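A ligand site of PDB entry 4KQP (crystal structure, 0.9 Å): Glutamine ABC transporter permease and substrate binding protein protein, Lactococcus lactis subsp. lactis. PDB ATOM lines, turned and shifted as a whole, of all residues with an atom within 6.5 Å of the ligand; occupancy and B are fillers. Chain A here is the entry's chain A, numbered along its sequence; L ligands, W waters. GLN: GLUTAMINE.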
ATOM      1  N   ASP A  15      11.826   0.390 -23.633  1.00  0.00           N
ATOM      2  CA  ASP A  15      11.888  -1.050 -23.759  1.00  0.00           C
ATOM      3  C   ASP A  15      11.026  -1.484 -24.938  1.00  0.00           C
ATOM      4  O   ASP A  15      10.126  -0.753 -25.369  1.00  0.00           O
ATOM      5  CB  ASP A  15      11.389  -1.687 -22.442  1.00  0.00           C
ATOM      6  CG  ASP A  15      11.920  -3.094 -22.189  1.00  0.00           C
ATOM      7  OD1 ASP A  15      12.384  -3.751 -23.149  1.00  0.00           O
ATOM      8  OD2 ASP A  15      11.843  -3.528 -21.026  1.00  0.00           O
ATOM      9  N   SER A  17       9.478  -4.632 -24.761  1.00  0.00           N
ATOM     10  CA  SER A  17       8.400  -5.449 -24.190  1.00  0.00           C
ATOM     11  C   SER A  17       8.420  -5.334 -22.677  1.00  0.00           C
ATOM     12  O   SER A  17       9.272  -5.913 -22.011  1.00  0.00           O
ATOM     13  CB  SER A  17       8.506  -6.906 -24.622  1.00  0.00           C
ATOM     14  OG  SER A  17       7.381  -7.648 -24.173  1.00  0.00           O
ATOM     15  N   PHE A  18       7.492  -4.546 -22.137  1.00  0.00           N
ATOM     16  CA  PHE A  18       7.410  -4.315 -20.699  1.00  0.00           C
ATOM     17  C   PHE A  18       5.961  -3.950 -20.345  1.00  0.00           C
ATOM     18  O   PHE A  18       5.694  -2.917 -19.736  1.00  0.00           O
ATOM     19  CB  PHE A  18       8.393  -3.222 -20.250  1.00  0.00           C
ATOM     20  CG  PHE A  18       8.734  -3.258 -18.775  1.00  0.00           C
ATOM     21  CD1 PHE A  18       9.268  -4.408 -18.226  1.00  0.00           C
ATOM     22  CD2 PHE A  18       8.576  -2.146 -17.963  1.00  0.00           C
ATOM     23  CE1 PHE A  18       9.626  -4.470 -16.895  1.00  0.00           C
ATOM     24  CE2 PHE A  18       8.932  -2.211 -16.619  1.00  0.00           C
ATOM     25  CZ  PHE A  18       9.467  -3.375 -16.087  1.00  0.00           C
ATOM     26  N   GLU A  22       5.155  -0.370 -21.593  1.00  0.00           N
ATOM     27  CA  GLU A  22       5.274  -0.235 -23.049  1.00  0.00           C
ATOM     28  C   GLU A  22       5.256  -1.620 -23.644  1.00  0.00           C
ATOM     29  O   GLU A  22       5.905  -2.536 -23.125  1.00  0.00           O
ATOM     30  CB  GLU A  22       6.541   0.501 -23.508  1.00  0.00           C
ATOM     31  CG  GLU A  22       7.833   0.045 -22.828  1.00  0.00           C
ATOM     32  CD  GLU A  22       8.070   0.751 -21.517  1.00  0.00           C
ATOM     33  OE1 GLU A  22       7.574   1.905 -21.391  1.00  0.00           O
ATOM     34  OE2 GLU A  22       8.766   0.207 -20.631  1.00  0.00           O
ATOM     35  N   PHE A  56      15.570  -2.216 -22.765  1.00  0.00           N
ATOM     36  CA  PHE A  56      15.944  -1.434 -21.592  1.00  0.00           C
ATOM     37  C   PHE A  56      17.427  -1.010 -21.615  1.00  0.00           C
ATOM     38  O   PHE A  56      17.739   0.180 -21.558  1.00  0.00           O
ATOM     39  CB  PHE A  56      15.622  -2.168 -20.279  1.00  0.00           C
ATOM     40  CG  PHE A  56      15.942  -1.341 -19.074  1.00  0.00           C
ATOM     41  CD1 PHE A  56      15.119  -0.294 -18.699  1.00  0.00           C
ATOM     42  CD2 PHE A  56      17.101  -1.553 -18.356  1.00  0.00           C
ATOM     43  CE1 PHE A  56      15.428   0.502 -17.613  1.00  0.00           C
ATOM     44  CE2 PHE A  56      17.430  -0.762 -17.275  1.00  0.00           C
ATOM     45  CZ  PHE A  56      16.592   0.264 -16.908  1.00  0.00           C
ATOM     46  N   SER A  73      10.710   4.028 -19.547  1.00  0.00           N
ATOM     47  CA  SER A  73      10.888   2.599 -19.763  1.00  0.00           C
ATOM     48  C   SER A  73      10.698   1.792 -18.484  1.00  0.00           C
ATOM     49  O   SER A  73      11.438   0.840 -18.232  1.00  0.00           O
ATOM     50  CB  SER A  73      12.301   2.362 -20.312  1.00  0.00           C
ATOM     51  OG  SER A  73      12.486   1.035 -20.760  1.00  0.00           O
ATOM     52  N   GLY A  74       9.724   2.179 -17.679  1.00  0.00           N
ATOM     53  CA  GLY A  74       9.518   1.542 -16.392  1.00  0.00           C
ATOM     54  C   GLY A  74      10.802   1.523 -15.573  1.00  0.00           C
ATOM     55  O   GLY A  74      11.141   0.512 -14.954  1.00  0.00           O
ATOM     56  N   MET A  75      11.504   2.644 -15.570  1.00  0.00           N
ATOM     57  CA  MET A  75      12.861   2.719 -15.049  1.00  0.00           C
ATOM     58  C   MET A  75      12.880   3.041 -13.560  1.00  0.00           C
ATOM     59  O   MET A  75      12.426   4.107 -13.133  1.00  0.00           O
ATOM     60  CB  MET A  75      13.632   3.801 -15.808  1.00  0.00           C
ATOM     61  CG  MET A  75      15.098   3.878 -15.439  1.00  0.00           C
ATOM     62  SD  MET A  75      15.805   5.288 -16.292  1.00  0.00           S
ATOM     63  CE  MET A  75      17.540   5.105 -15.929  1.00  0.00           C
ATOM     64  N   SER A  76      13.437   2.128 -12.782  1.00  0.00           N
ATOM     65  CA  SER A  76      13.574   2.359 -11.348  1.00  0.00           C
ATOM     66  C   SER A  76      14.541   3.503 -11.066  1.00  0.00           C
ATOM     67  O   SER A  76      15.592   3.640 -11.721  1.00  0.00           O
ATOM     68  CB  SER A  76      14.066   1.076 -10.668  1.00  0.00           C
ATOM     69  OG  SER A  76      13.144   0.012 -10.830  1.00  0.00           O
ATOM     70  N   ILE A  77      14.177   4.300 -10.065  1.00  0.00           N
ATOM     71  CA  ILE A  77      15.026   5.376  -9.551  1.00  0.00           C
ATOM     72  C   ILE A  77      15.939   4.788  -8.489  1.00  0.00           C
ATOM     73  O   ILE A  77      15.457   4.217  -7.507  1.00  0.00           O
ATOM     74  CB  ILE A  77      14.170   6.526  -8.959  1.00  0.00           C
ATOM     75  CG1 ILE A  77      13.205   7.074 -10.009  1.00  0.00           C
ATOM     76  CG2 ILE A  77      15.082   7.620  -8.417  1.00  0.00           C
ATOM     77  CD1 ILE A  77      12.222   8.097  -9.466  1.00  0.00           C
ATOM     78  N   ARG A  81      22.093   5.080 -10.166  1.00  0.00           N
ATOM     79  CA  ARG A  81      21.744   5.607 -11.482  1.00  0.00           C
ATOM     80  C   ARG A  81      21.778   7.135 -11.497  1.00  0.00           C
ATOM     81  O   ARG A  81      22.062   7.738 -12.530  1.00  0.00           O
ATOM     82  CB  ARG A  81      20.389   5.081 -11.926  1.00  0.00           C
ATOM     83  CG  ARG A  81      20.465   3.634 -12.375  1.00  0.00           C
ATOM     84  CD  ARG A  81      19.088   3.035 -12.560  1.00  0.00           C
ATOM     85  NE  ARG A  81      19.175   1.656 -13.021  1.00  0.00           N
ATOM     86  CZ  ARG A  81      18.125   0.917 -13.345  1.00  0.00           C
ATOM     87  NH1 ARG A  81      16.911   1.414 -13.255  1.00  0.00           N
ATOM     88  NH2 ARG A  81      18.298  -0.323 -13.781  1.00  0.00           N
ATOM     89  N   SER A  94       7.356   0.102  -7.818  1.00  0.00           N
ATOM     90  CA  SER A  94       7.531  -1.312  -8.097  1.00  0.00           C
ATOM     91  C   SER A  94       8.366  -2.026  -7.055  1.00  0.00           C
ATOM     92  O   SER A  94       9.238  -1.445  -6.405  1.00  0.00           O
ATOM     93  CB  SER A  94       8.158  -1.534  -9.481  1.00  0.00           C
ATOM     94  OG  SER A  94       9.561  -1.330  -9.458  1.00  0.00           O
ATOM     95  N   LEU A  96      10.388  -6.095  -6.842  1.00  0.00           N
ATOM     96  CA  LEU A  96      10.922  -7.196  -7.647  1.00  0.00           C
ATOM     97  C   LEU A  96      10.284  -8.515  -7.203  1.00  0.00           C
ATOM     98  O   LEU A  96      10.097  -8.739  -6.006  1.00  0.00           O
ATOM     99  CB  LEU A  96      12.428  -7.300  -7.461  1.00  0.00           C
ATOM    100  CG  LEU A  96      13.229  -6.080  -7.927  1.00  0.00           C
ATOM    101  CD1 LEU A  96      14.641  -6.135  -7.376  1.00  0.00           C
ATOM    102  CD2 LEU A  96      13.265  -6.027  -9.443  1.00  0.00           C
ATOM    103  N   LYS A 121      16.538  -9.791 -17.305  1.00  0.00           N
ATOM    104  CA  LYS A 121      16.827  -8.953 -18.459  1.00  0.00           C
ATOM    105  C   LYS A 121      18.105  -8.147 -18.253  1.00  0.00           C
ATOM    106  O   LYS A 121      18.369  -7.605 -17.175  1.00  0.00           O
ATOM    107  CB  LYS A 121      15.666  -8.006 -18.717  1.00  0.00           C
ATOM    108  CG  LYS A 121      14.435  -8.704 -19.205  1.00  0.00           C
ATOM    109  CD  LYS A 121      13.193  -7.885 -18.977  1.00  0.00           C
ATOM    110  CE  LYS A 121      13.172  -6.624 -19.805  1.00  0.00           C
ATOM    111  NZ  LYS A 121      11.948  -5.815 -19.554  1.00  0.00           N
ATOM    112  N   GLY A 123      20.814  -5.589 -17.794  1.00  0.00           N
ATOM    113  CA  GLY A 123      20.924  -4.226 -17.301  1.00  0.00           C
ATOM    114  C   GLY A 123      19.885  -3.781 -16.294  1.00  0.00           C
ATOM    115  O   GLY A 123      19.872  -2.626 -15.883  1.00  0.00           O
ATOM    116  N   THR A 124      18.998  -4.687 -15.884  1.00  0.00           N
ATOM    117  CA  THR A 124      17.877  -4.320 -15.032  1.00  0.00           C
ATOM    118  C   THR A 124      18.143  -4.516 -13.541  1.00  0.00           C
ATOM    119  O   THR A 124      19.084  -5.205 -13.130  1.00  0.00           O
ATOM    120  CB  THR A 124      16.625  -5.137 -15.391  1.00  0.00           C
ATOM    121  OG1 THR A 124      16.862  -6.529 -15.127  1.00  0.00           O
ATOM    122  CG2 THR A 124      16.201  -4.889 -16.842  1.00  0.00           C
ATOM    123  N   ALA A 125      17.255  -3.938 -12.736  1.00  0.00           N
ATOM    124  CA  ALA A 125      17.266  -4.149 -11.302  1.00  0.00           C
ATOM    125  C   ALA A 125      17.126  -5.643 -10.956  1.00  0.00           C
ATOM    126  O   ALA A 125      17.711  -6.104  -9.980  1.00  0.00           O
ATOM    127  CB  ALA A 125      16.162  -3.352 -10.661  1.00  0.00           C
ATOM    128  N   SER A 126      16.352  -6.379 -11.753  1.00  0.00           N
ATOM    129  CA  SER A 126      16.226  -7.815 -11.553  1.00  0.00           C
ATOM    130  C   SER A 126      17.557  -8.526 -11.758  1.00  0.00           C
ATOM    131  O   SER A 126      17.940  -9.392 -10.966  1.00  0.00           O
ATOM    132  CB  SER A 126      15.208  -8.407 -12.528  1.00  0.00           C
ATOM    133  OG  SER A 126      13.885  -8.071 -12.191  1.00  0.00           O
ATOM    134  N   ASP A 128      20.492  -7.140 -11.417  1.00  0.00           N
ATOM    135  CA  ASP A 128      21.375  -6.743 -10.332  1.00  0.00           C
ATOM    136  C   ASP A 128      21.101  -7.580  -9.081  1.00  0.00           C
ATOM    137  O   ASP A 128      22.030  -8.066  -8.426  1.00  0.00           O
ATOM    138  CB  ASP A 128      21.227  -5.257 -10.003  1.00  0.00           C
ATOM    139  CG  ASP A 128      21.617  -4.343 -11.167  1.00  0.00           C
ATOM    140  OD1 ASP A 128      22.473  -4.741 -11.985  1.00  0.00           O
ATOM    141  OD2 ASP A 128      21.082  -3.207 -11.250  1.00  0.00           O
ATOM    142  N   ASP A 164      11.488 -10.330 -12.408  1.00  0.00           N
ATOM    143  CA  ASP A 164      11.056  -9.152 -13.141  1.00  0.00           C
ATOM    144  C   ASP A 164      10.282  -8.277 -12.154  1.00  0.00           C
ATOM    145  O   ASP A 164      10.068  -8.646 -10.974  1.00  0.00           O
ATOM    146  CB  ASP A 164      10.182  -9.568 -14.347  1.00  0.00           C
ATOM    147  CG  ASP A 164      10.145  -8.550 -15.485  1.00  0.00           C
ATOM    148  OD1 ASP A 164      10.595  -7.390 -15.312  1.00  0.00           O
ATOM    149  OD2 ASP A 164       9.627  -8.930 -16.563  1.00  0.00           O
ATOM    150  N   ASP A 165       9.857  -7.114 -12.618  1.00  0.00           N
ATOM    151  CA  ASP A 165       9.093  -6.221 -11.757  1.00  0.00           C
ATOM    152  C   ASP A 165       7.702  -6.798 -11.477  1.00  0.00           C
ATOM    153  O   ASP A 165       7.023  -7.327 -12.365  1.00  0.00           O
ATOM    154  CB  ASP A 165       8.956  -4.834 -12.397  1.00  0.00           C
ATOM    155  CG  ASP A 165      10.246  -4.008 -12.354  1.00  0.00           C
ATOM    156  OD1 ASP A 165      11.298  -4.505 -11.896  1.00  0.00           O
ATOM    157  OD2 ASP A 165      10.161  -2.831 -12.778  1.00  0.00           O
ATOM    158  N   ASP A 188      11.309  -2.172  -4.073  1.00  0.00           N
ATOM    159  CA  ASP A 188      12.233  -1.598  -5.032  1.00  0.00           C
ATOM    160  C   ASP A 188      11.902  -0.179  -5.495  1.00  0.00           C
ATOM    161  O   ASP A 188      12.321   0.234  -6.568  1.00  0.00           O
ATOM    162  CB  ASP A 188      12.421  -2.519  -6.250  1.00  0.00           C
ATOM    163  CG  ASP A 188      13.738  -2.262  -6.991  1.00  0.00           C
ATOM    164  OD1 ASP A 188      14.740  -1.947  -6.334  1.00  0.00           O
ATOM    165  OD2 ASP A 188      13.763  -2.388  -8.251  1.00  0.00           O
ATOM    166  N   GLN A 190      10.551   3.426  -6.768  1.00  0.00           N
ATOM    167  CA  GLN A 190       9.680   4.139  -7.705  1.00  0.00           C
ATOM    168  C   GLN A 190      10.242   4.086  -9.132  1.00  0.00           C
ATOM    169  O   GLN A 190      11.412   3.740  -9.333  1.00  0.00           O
ATOM    170  CB  GLN A 190       9.487   5.593  -7.243  1.00  0.00           C
ATOM    171  CG  GLN A 190       8.662   5.693  -5.933  1.00  0.00           C
ATOM    172  CD  GLN A 190       8.715   7.057  -5.272  1.00  0.00           C
ATOM    173  OE1 GLN A 190       9.788   7.605  -5.019  1.00  0.00           O
ATOM    174  NE2 GLN A 190       7.545   7.612  -4.971  1.00  0.00           N
ATOM    175  N   TYR A 191       9.393   4.415 -10.099  1.00  0.00           N
ATOM    176  CA  TYR A 191       9.794   4.636 -11.492  1.00  0.00           C
ATOM    177  C   TYR A 191       9.947   6.131 -11.762  1.00  0.00           C
ATOM    178  O   TYR A 191       9.188   6.952 -11.225  1.00  0.00           O
ATOM    179  CB  TYR A 191       8.735   4.127 -12.468  1.00  0.00           C
ATOM    180  CG  TYR A 191       8.552   2.634 -12.614  1.00  0.00           C
ATOM    181  CD1 TYR A 191       9.399   1.703 -12.017  1.00  0.00           C
ATOM    182  CD2 TYR A 191       7.521   2.160 -13.409  1.00  0.00           C
ATOM    183  CE1 TYR A 191       9.192   0.316 -12.215  1.00  0.00           C
ATOM    184  CE2 TYR A 191       7.315   0.810 -13.612  1.00  0.00           C
ATOM    185  CZ  TYR A 191       8.149  -0.105 -13.006  1.00  0.00           C
ATOM    186  OH  TYR A 191       7.902  -1.444 -13.235  1.00  0.00           O
HETATM  187  N   GLN L   1      12.362  -1.306 -13.219  1.00  0.00           N
HETATM  188  CA  GLN L   1      13.485  -2.166 -13.688  1.00  0.00           C
HETATM  189  C   GLN L   1      14.746  -1.340 -13.899  1.00  0.00           C
HETATM  190  O   GLN L   1      14.657  -0.092 -13.918  1.00  0.00           O
HETATM  191  CB  GLN L   1      13.102  -2.925 -14.960  1.00  0.00           C
HETATM  192  CG  GLN L   1      12.923  -2.053 -16.191  1.00  0.00           C
HETATM  193  CD  GLN L   1      12.598  -2.852 -17.441  1.00  0.00           C
HETATM  194  OE1 GLN L   1      12.875  -4.057 -17.516  1.00  0.00           O
HETATM  195  NE2 GLN L   1      12.057  -2.172 -18.441  1.00  0.00           N
HETATM  196  OXT GLN L   1      15.814  -1.956 -14.047  1.00  0.00           O
HETATM  197  O   HOH W   1      13.019  -6.263 -15.682  1.00  0.00           O
HETATM  198  O   HOH W   2      13.637  -5.532 -13.052  1.00  0.00           O
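OD2 of Asp 165 lies within hydrogen-bond range of OH of Tyr 191 (2.7 Å).
O of Ser 76 lies within hydrogen-bond range of NH1 of Arg 81, at 3.0 Å.
The guanidinium group (NH2) of Arg 81 lies within hydrogen-bond range of the backbone carbonyl oxygen (O) of Gly 123, 3.5 Å away.
OD2 of Asp 15 lies within salt-bridge range of NZ of Lys 121.
The side-chain hydroxyl (OG1) of Thr 124 sits at hydrogen-bond distance from the backbone carbonyl oxygen (O) of Lys 121 (2.8 Å).
The backbone NH of Asp 15 lies within hydrogen-bond range of the side-chain hydroxyl of Ser 73.
The side-chain carboxylate (OD1) of Asp 15 sits at hydrogen-bond distance from the backbone NH (N) of Ser 17, at 3.4 Å.
The side-chain hydroxyl (OG1) of Thr 124 lies close to the backbone NH (N) of Ser 126 (3.4 Å).
The side-chain carboxylate (OD2) of Asp 165 lies within salt-bridge range of a nitrogen (N) of the ligand.
The backbone NH (N) of Ser 76 lies within hydrogen-bond range of an oxygen (O) of the ligand, 2.8 Å away.
OG of Ser 76 is in hydrogen-bond range of N of the ligand, at 2.8 Å.
An oxygen (OXT) of the ligand sits at hydrogen-bond distance from the backbone NH (N) of Ala 125 (2.8 Å).
The guanidinium group (NH1) of Arg 81 lies within salt-bridge range of an oxygen (O) of the ligand, 2.8 Å away.
O of Gly 74 sits at hydrogen-bond distance from N of the ligand (2.8 Å).
The side-chain amino group of Lys 121 is in hydrogen-bond range of an oxygen (OE1) of the ligand, at 2.8 Å.
OD2 of Asp 15 lies within hydrogen-bond range of NE2 of the ligand (2.9 Å).
A nitrogen (NE2) of the ligand is in hydrogen-bond range of the backbone carbonyl oxygen (O) of Ser 73.
Residues that only touch the ligand: Phe 18, Phe 56, Met 75, Thr 124 and Tyr 191.
Hydrophobic or aromatic side chains that line the ligand: Phe 18, Phe 56, Ala 125 and Tyr 191.
Of the 24 residues printed, 13 come within 4 Å of the ligand.
The nearest printed residue that does not touch the ligand is Gly 123 (4.5 Å).
Water W1 lies within hydrogen-bond range of OD1 of Asp 164 (2.7 Å) and OE1 of the ligand (2.9 Å).
Water W2 bridges the side-chain hydroxyl (OG) of Ser 126 (2.7 Å) and the side-chain carboxylate (OD1) of Asp 165 (2.8 Å).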
